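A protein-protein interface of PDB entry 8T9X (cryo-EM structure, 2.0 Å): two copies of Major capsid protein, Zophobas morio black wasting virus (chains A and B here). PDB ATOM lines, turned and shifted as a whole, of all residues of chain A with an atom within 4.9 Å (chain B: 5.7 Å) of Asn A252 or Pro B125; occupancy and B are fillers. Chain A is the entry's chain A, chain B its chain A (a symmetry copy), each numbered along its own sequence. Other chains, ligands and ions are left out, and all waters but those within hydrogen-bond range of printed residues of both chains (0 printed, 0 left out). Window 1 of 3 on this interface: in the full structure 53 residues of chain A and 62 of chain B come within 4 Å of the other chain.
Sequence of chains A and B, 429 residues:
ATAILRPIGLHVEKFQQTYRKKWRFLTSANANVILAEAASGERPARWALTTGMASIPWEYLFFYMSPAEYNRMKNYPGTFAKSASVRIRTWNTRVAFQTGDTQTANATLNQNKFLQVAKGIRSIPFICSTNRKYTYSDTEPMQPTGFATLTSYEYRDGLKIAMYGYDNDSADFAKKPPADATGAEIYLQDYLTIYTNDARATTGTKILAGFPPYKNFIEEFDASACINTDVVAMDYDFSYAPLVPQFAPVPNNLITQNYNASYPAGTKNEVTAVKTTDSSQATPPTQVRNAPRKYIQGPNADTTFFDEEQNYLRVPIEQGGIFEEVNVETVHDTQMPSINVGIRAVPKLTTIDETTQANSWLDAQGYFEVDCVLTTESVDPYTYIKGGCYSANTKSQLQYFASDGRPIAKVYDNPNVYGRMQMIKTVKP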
ATOM      1  N   VAL A 250      21.957  -1.582 -26.589  1.00  0.00           N
ATOM      2  CA  VAL A 250      21.530  -2.695 -27.430  1.00  0.00           C
ATOM      3  C   VAL A 250      20.103  -3.025 -27.010  1.00  0.00           C
ATOM      4  O   VAL A 250      19.860  -3.310 -25.830  1.00  0.00           O
ATOM      5  CB  VAL A 250      22.463  -3.909 -27.296  1.00  0.00           C
ATOM      6  CG1 VAL A 250      21.793  -5.154 -27.853  1.00  0.00           C
ATOM      7  CG2 VAL A 250      23.785  -3.651 -28.003  1.00  0.00           C
ATOM      8  N   PRO A 251      19.132  -2.983 -27.922  1.00  0.00           N
ATOM      9  CA  PRO A 251      17.728  -3.196 -27.531  1.00  0.00           C
ATOM     10  C   PRO A 251      17.485  -4.647 -27.141  1.00  0.00           C
ATOM     11  O   PRO A 251      17.730  -5.562 -27.928  1.00  0.00           O
ATOM     12  CB  PRO A 251      16.945  -2.810 -28.792  1.00  0.00           C
ATOM     13  CG  PRO A 251      17.922  -2.091 -29.666  1.00  0.00           C
ATOM     14  CD  PRO A 251      19.259  -2.659 -29.349  1.00  0.00           C
ATOM     15  N   ASN A 252      16.984  -4.850 -25.919  1.00  0.00           N
ATOM     16  CA  ASN A 252      16.749  -6.193 -25.398  1.00  0.00           C
ATOM     17  C   ASN A 252      15.562  -6.895 -26.038  1.00  0.00           C
ATOM     18  O   ASN A 252      15.453  -8.117 -25.908  1.00  0.00           O
ATOM     19  CB  ASN A 252      16.546  -6.149 -23.882  1.00  0.00           C
ATOM     20  CG  ASN A 252      17.845  -6.204 -23.124  1.00  0.00           C
ATOM     21  OD1 ASN A 252      18.899  -6.468 -23.700  1.00  0.00           O
ATOM     22  ND2 ASN A 252      17.782  -5.968 -21.822  1.00  0.00           N
ATOM     23  N   ASN A 253      14.666  -6.166 -26.709  1.00  0.00           N
ATOM     24  CA  ASN A 253      13.584  -6.824 -27.431  1.00  0.00           C
ATOM     25  C   ASN A 253      14.104  -7.700 -28.563  1.00  0.00           C
ATOM     26  O   ASN A 253      13.389  -8.602 -29.011  1.00  0.00           O
ATOM     27  CB  ASN A 253      12.601  -5.790 -27.976  1.00  0.00           C
ATOM     28  CG  ASN A 253      13.152  -5.028 -29.163  1.00  0.00           C
ATOM     29  OD1 ASN A 253      14.159  -4.340 -29.051  1.00  0.00           O
ATOM     30  ND2 ASN A 253      12.494  -5.152 -30.306  1.00  0.00           N
ATOM     31  N   LEU A 254      15.326  -7.458 -29.032  1.00  0.00           N
ATOM     32  CA  LEU A 254      15.955  -8.326 -30.016  1.00  0.00           C
ATOM     33  C   LEU A 254      16.536  -9.593 -29.401  1.00  0.00           C
ATOM     34  O   LEU A 254      16.932 -10.493 -30.146  1.00  0.00           O
ATOM     35  CB  LEU A 254      17.060  -7.567 -30.754  1.00  0.00           C
ATOM     36  CG  LEU A 254      16.666  -6.248 -31.420  1.00  0.00           C
ATOM     37  CD1 LEU A 254      17.893  -5.542 -31.962  1.00  0.00           C
ATOM     38  CD2 LEU A 254      15.660  -6.491 -32.526  1.00  0.00           C
ATOM     39  N   ILE A 255      16.596  -9.687 -28.073  1.00  0.00           N
ATOM     40  CA  ILE A 255      17.232 -10.821 -27.414  1.00  0.00           C
ATOM     41  C   ILE A 255      16.250 -11.556 -26.508  1.00  0.00           C
ATOM     42  O   ILE A 255      16.362 -12.771 -26.319  1.00  0.00           O
ATOM     43  CB  ILE A 255      18.463 -10.362 -26.609  1.00  0.00           C
ATOM     44  CG1 ILE A 255      19.271  -9.327 -27.395  1.00  0.00           C
ATOM     45  CG2 ILE A 255      19.340 -11.541 -26.245  1.00  0.00           C
ATOM     46  CD1 ILE A 255      20.439  -8.764 -26.632  1.00  0.00           C
ATOM     47  N   THR A 256      15.272 -10.840 -25.957  1.00  0.00           N
ATOM     48  CA  THR A 256      14.417 -11.378 -24.907  1.00  0.00           C
ATOM     49  C   THR A 256      12.958 -11.359 -25.336  1.00  0.00           C
ATOM     50  O   THR A 256      12.544 -10.546 -26.163  1.00  0.00           O
ATOM     51  CB  THR A 256      14.534 -10.587 -23.589  1.00  0.00           C
ATOM     52  OG1 THR A 256      13.869  -9.326 -23.724  1.00  0.00           O
ATOM     53  CG2 THR A 256      15.972 -10.335 -23.244  1.00  0.00           C
ATOM     54  N   TYR A 259      10.698  -8.279 -22.893  1.00  0.00           N
ATOM     55  CA  TYR A 259      11.143  -6.892 -22.986  1.00  0.00           C
ATOM     56  C   TYR A 259      10.090  -5.899 -22.507  1.00  0.00           C
ATOM     57  O   TYR A 259      10.445  -4.790 -22.095  1.00  0.00           O
ATOM     58  CB  TYR A 259      11.542  -6.577 -24.427  1.00  0.00           C
ATOM     59  CG  TYR A 259      10.399  -6.687 -25.403  1.00  0.00           C
ATOM     60  CD1 TYR A 259       9.589  -5.595 -25.679  1.00  0.00           C
ATOM     61  CD2 TYR A 259      10.121  -7.886 -26.040  1.00  0.00           C
ATOM     62  CE1 TYR A 259       8.543  -5.694 -26.563  1.00  0.00           C
ATOM     63  CE2 TYR A 259       9.079  -7.992 -26.929  1.00  0.00           C
ATOM     64  CZ  TYR A 259       8.294  -6.893 -27.187  1.00  0.00           C
ATOM     65  OH  TYR A 259       7.249  -6.998 -28.072  1.00  0.00           O
ATOM     66  N   ALA A 392      24.292   0.924 -20.975  1.00  0.00           N
ATOM     67  CA  ALA A 392      23.265   0.126 -20.323  1.00  0.00           C
ATOM     68  C   ALA A 392      21.907   0.777 -20.538  1.00  0.00           C
ATOM     69  O   ALA A 392      21.794   2.005 -20.593  1.00  0.00           O
ATOM     70  CB  ALA A 392      23.564  -0.013 -18.830  1.00  0.00           C
ATOM     71  N   ASN A 393      20.866  -0.048 -20.678  1.00  0.00           N
ATOM     72  CA  ASN A 393      19.542   0.499 -20.954  1.00  0.00           C
ATOM     73  C   ASN A 393      18.967   1.262 -19.766  1.00  0.00           C
ATOM     74  O   ASN A 393      17.979   1.981 -19.927  1.00  0.00           O
ATOM     75  CB  ASN A 393      18.583  -0.610 -21.403  1.00  0.00           C
ATOM     76  CG  ASN A 393      18.399  -1.702 -20.363  1.00  0.00           C
ATOM     77  OD1 ASN A 393      18.896  -1.614 -19.244  1.00  0.00           O
ATOM     78  ND2 ASN A 393      17.682  -2.749 -20.743  1.00  0.00           N
ATOM     79  N   THR A 394      19.566   1.132 -18.582  1.00  0.00           N
ATOM     80  CA  THR A 394      19.185   1.975 -17.455  1.00  0.00           C
ATOM     81  C   THR A 394      19.642   3.417 -17.628  1.00  0.00           C
ATOM     82  O   THR A 394      19.268   4.267 -16.815  1.00  0.00           O
ATOM     83  CB  THR A 394      19.741   1.405 -16.149  1.00  0.00           C
ATOM     84  OG1 THR A 394      21.151   1.188 -16.279  1.00  0.00           O
ATOM     85  CG2 THR A 394      19.055   0.093 -15.802  1.00  0.00           C
ATOM     86  N   PRO B  44      12.492 -13.717 -29.883  1.00  0.00           N
ATOM     87  CA  PRO B  44      13.201 -13.526 -31.149  1.00  0.00           C
ATOM     88  C   PRO B  44      14.295 -14.566 -31.327  1.00  0.00           C
ATOM     89  O   PRO B  44      14.745 -15.208 -30.376  1.00  0.00           O
ATOM     90  CB  PRO B  44      13.792 -12.121 -31.021  1.00  0.00           C
ATOM     91  CG  PRO B  44      13.854 -11.849 -29.553  1.00  0.00           C
ATOM     92  CD  PRO B  44      12.999 -12.840 -28.817  1.00  0.00           C
ATOM     93  N   SER B 123      21.409  -9.653 -12.416  1.00  0.00           N
ATOM     94  CA  SER B 123      20.852  -8.308 -12.335  1.00  0.00           C
ATOM     95  C   SER B 123      21.599  -7.281 -13.181  1.00  0.00           C
ATOM     96  O   SER B 123      21.215  -6.108 -13.177  1.00  0.00           O
ATOM     97  CB  SER B 123      20.818  -7.854 -10.874  1.00  0.00           C
ATOM     98  OG  SER B 123      22.077  -7.367 -10.451  1.00  0.00           O
ATOM     99  N   ILE B 124      22.633  -7.682 -13.915  1.00  0.00           N
ATOM    100  CA  ILE B 124      23.407  -6.738 -14.721  1.00  0.00           C
ATOM    101  C   ILE B 124      22.580  -6.326 -15.937  1.00  0.00           C
ATOM    102  O   ILE B 124      22.208  -7.180 -16.753  1.00  0.00           O
ATOM    103  CB  ILE B 124      24.762  -7.333 -15.130  1.00  0.00           C
ATOM    104  CG1 ILE B 124      25.581  -7.675 -13.882  1.00  0.00           C
ATOM    105  CG2 ILE B 124      25.517  -6.368 -16.028  1.00  0.00           C
ATOM    106  CD1 ILE B 124      26.932  -8.284 -14.169  1.00  0.00           C
ATOM    107  N   PRO B 125      22.277  -5.035 -16.096  1.00  0.00           N
ATOM    108  CA  PRO B 125      21.297  -4.623 -17.118  1.00  0.00           C
ATOM    109  C   PRO B 125      21.694  -4.937 -18.550  1.00  0.00           C
ATOM    110  O   PRO B 125      20.813  -5.212 -19.372  1.00  0.00           O
ATOM    111  CB  PRO B 125      21.178  -3.108 -16.898  1.00  0.00           C
ATOM    112  CG  PRO B 125      21.719  -2.862 -15.535  1.00  0.00           C
ATOM    113  CD  PRO B 125      22.768  -3.896 -15.307  1.00  0.00           C
ATOM    114  N   PHE B 126      22.979  -4.890 -18.888  1.00  0.00           N
ATOM    115  CA  PHE B 126      23.399  -5.066 -20.274  1.00  0.00           C
ATOM    116  C   PHE B 126      23.798  -6.496 -20.608  1.00  0.00           C
ATOM    117  O   PHE B 126      24.220  -6.756 -21.738  1.00  0.00           O
ATOM    118  CB  PHE B 126      24.558  -4.118 -20.607  1.00  0.00           C
ATOM    119  CG  PHE B 126      25.616  -4.058 -19.550  1.00  0.00           C
ATOM    120  CD1 PHE B 126      26.668  -4.954 -19.553  1.00  0.00           C
ATOM    121  CD2 PHE B 126      25.557  -3.109 -18.547  1.00  0.00           C
ATOM    122  CE1 PHE B 126      27.641  -4.901 -18.582  1.00  0.00           C
ATOM    123  CE2 PHE B 126      26.527  -3.054 -17.570  1.00  0.00           C
ATOM    124  CZ  PHE B 126      27.572  -3.952 -17.587  1.00  0.00           C
ATOM    125  N   ILE B 127      23.674  -7.424 -19.671  1.00  0.00           N
ATOM    126  CA  ILE B 127      23.968  -8.829 -19.917  1.00  0.00           C
ATOM    127  C   ILE B 127      22.653  -9.592 -19.853  1.00  0.00           C
ATOM    128  O   ILE B 127      22.029  -9.689 -18.793  1.00  0.00           O
ATOM    129  CB  ILE B 127      24.984  -9.380 -18.909  1.00  0.00           C
ATOM    130  CG1 ILE B 127      26.305  -8.614 -19.018  1.00  0.00           C
ATOM    131  CG2 ILE B 127      25.193 -10.868 -19.132  1.00  0.00           C
ATOM    132  CD1 ILE B 127      27.330  -9.010 -17.991  1.00  0.00           C
ATOM    133  N   CYS B 128      22.227 -10.139 -20.986  1.00  0.00           N
ATOM    134  CA  CYS B 128      21.008 -10.938 -21.043  1.00  0.00           C
ATOM    135  C   CYS B 128      21.362 -12.400 -20.791  1.00  0.00           C
ATOM    136  O   CYS B 128      22.026 -13.033 -21.615  1.00  0.00           O
ATOM    137  CB  CYS B 128      20.319 -10.760 -22.390  1.00  0.00           C
ATOM    138  SG  CYS B 128      18.904 -11.833 -22.616  1.00  0.00           S
ATOM    139  N   SER B 279      11.596  -2.201 -23.557  1.00  0.00           N
ATOM    140  CA  SER B 279      12.928  -2.050 -24.129  1.00  0.00           C
ATOM    141  C   SER B 279      12.896  -1.925 -25.648  1.00  0.00           C
ATOM    142  O   SER B 279      13.866  -1.436 -26.233  1.00  0.00           O
ATOM    143  CB  SER B 279      13.816  -3.221 -23.705  1.00  0.00           C
ATOM    144  OG  SER B 279      13.727  -4.293 -24.619  1.00  0.00           O
ATOM    145  N   ASN B 416      16.774 -10.172 -16.694  1.00  0.00           N
ATOM    146  CA  ASN B 416      16.374  -8.913 -16.084  1.00  0.00           C
ATOM    147  C   ASN B 416      15.937  -7.912 -17.147  1.00  0.00           C
ATOM    148  O   ASN B 416      16.414  -7.926 -18.284  1.00  0.00           O
ATOM    149  CB  ASN B 416      17.512  -8.331 -15.240  1.00  0.00           C
ATOM    150  CG  ASN B 416      18.616  -7.703 -16.074  1.00  0.00           C
ATOM    151  OD1 ASN B 416      18.494  -6.572 -16.536  1.00  0.00           O
ATOM    152  ND2 ASN B 416      19.703  -8.431 -16.257  1.00  0.00           N
ATOM    153  N   VAL B 417      15.001  -7.051 -16.766  1.00  0.00           N
ATOM    154  CA  VAL B 417      14.560  -5.936 -17.592  1.00  0.00           C
ATOM    155  C   VAL B 417      14.960  -4.656 -16.876  1.00  0.00           C
ATOM    156  O   VAL B 417      14.437  -4.348 -15.798  1.00  0.00           O
ATOM    157  CB  VAL B 417      13.048  -5.993 -17.863  1.00  0.00           C
ATOM    158  CG1 VAL B 417      12.762  -6.991 -18.956  1.00  0.00           C
ATOM    159  CG2 VAL B 417      12.282  -6.371 -16.608  1.00  0.00           C
ATOM    160  N   TYR B 418      15.906  -3.926 -17.465  1.00  0.00           N
ATOM    161  CA  TYR B 418      16.478  -2.730 -16.846  1.00  0.00           C
ATOM    162  C   TYR B 418      17.021  -3.037 -15.453  1.00  0.00           C
ATOM    163  O   TYR B 418      16.900  -2.235 -14.526  1.00  0.00           O
ATOM    164  CB  TYR B 418      15.458  -1.593 -16.796  1.00  0.00           C
ATOM    165  CG  TYR B 418      15.011  -1.124 -18.155  1.00  0.00           C
ATOM    166  CD1 TYR B 418      15.719  -0.142 -18.836  1.00  0.00           C
ATOM    167  CD2 TYR B 418      13.888  -1.661 -18.762  1.00  0.00           C
ATOM    168  CE1 TYR B 418      15.316   0.292 -20.080  1.00  0.00           C
ATOM    169  CE2 TYR B 418      13.478  -1.234 -20.008  1.00  0.00           C
ATOM    170  CZ  TYR B 418      14.197  -0.255 -20.661  1.00  0.00           C
ATOM    171  OH  TYR B 418      13.796   0.177 -21.899  1.00  0.00           O
ATOM    172  N   GLY B 419      17.623  -4.214 -15.304  1.00  0.00           N
ATOM    173  CA  GLY B 419      18.154  -4.618 -14.022  1.00  0.00           C
ATOM    174  C   GLY B 419      17.124  -5.052 -13.005  1.00  0.00           C
ATOM    175  O   GLY B 419      17.455  -5.160 -11.823  1.00  0.00           O
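Of chain B, only Pro B125 (3.97 Å) and Ser B279 (3.5 Å) come within 4 Å of Asn A252. Printed residues of chain A within 4 Å of Pro B125: Asn A252 (3.97 Å), Asn A393 (3.6 Å) and Thr A394 (3.99 Å). Of the printed residues of chain B, Asn A393 touches Pro B125 and Tyr B418. Of the printed residues of chain A, Phe B126 touches Ala A392 (3.7 Å). Val A250 touches none of the printed residues of chain B. Asn B416 touches none of the printed residues of chain A. The nearest residue of chain B that does not touch Asn A252 is Asn B416 (4.3 Å).
OG of Ser B279 lies within hydrogen-bond range of N of Asn A253, at 3.0 Å. O of Tyr A259 sits at hydrogen-bond distance from N of Ser B279 (3.2 Å).
No position is printed for both chains. Of the 15 pairs that touch across the chains among the printed residues, none has its exchanged pair printed and touching as well.
The backbone carbonyl oxygen (O) of Asn A252 lies within hydrogen-bond range of the side-chain hydroxyl (OG1) of Thr A256 (3.0 Å). ND2 of Asn A252 sits close to ND2 of Asn A393, at 3.4 Å. The side-chain hydroxyl (OG1) of Thr A256 is in hydrogen-bond range of the backbone NH (N) of Tyr A259, 3.4 Å away.
O of Pro B125 touches ND2 of Asn A252, at 3.97 Å. OG of Ser B279 touches CB of Asn A252 (3.5 Å). Asn A253 touches Pro B44. Leu A254 touches Pro B44. Ile A255 touches Pro B44 (N to CG, 3.8 Å). SG of Cys B128 touches CG2 of Ile A255, at 3.7 Å. CD of Pro B44 touches O of Thr A256, 3.5 Å away. Pro B125 touches Asn A393 (CB to OD1, 3.6 Å). CG2 of Thr A394 touches CG of Pro B125, 3.99 Å away. Thr A394 touches Tyr B418 (CG2 to O, 3.4 Å).
Of the 11 printed residues of chain A, 9 touch a printed residue of chain B. Printed residues of chain A that touch a printed residue of chain B: Asn A252, Asn A253, Leu A254, Ile A255, Thr A256, Tyr A259, Ala A392, Asn A393 and Thr A394. Hydrophobic or aromatic side chains of chain B that line the printed part of chain A: Pro B44, Pro B125, Phe B126 and Tyr B418. Among the printed residues, 15 pairs touch across the chains.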
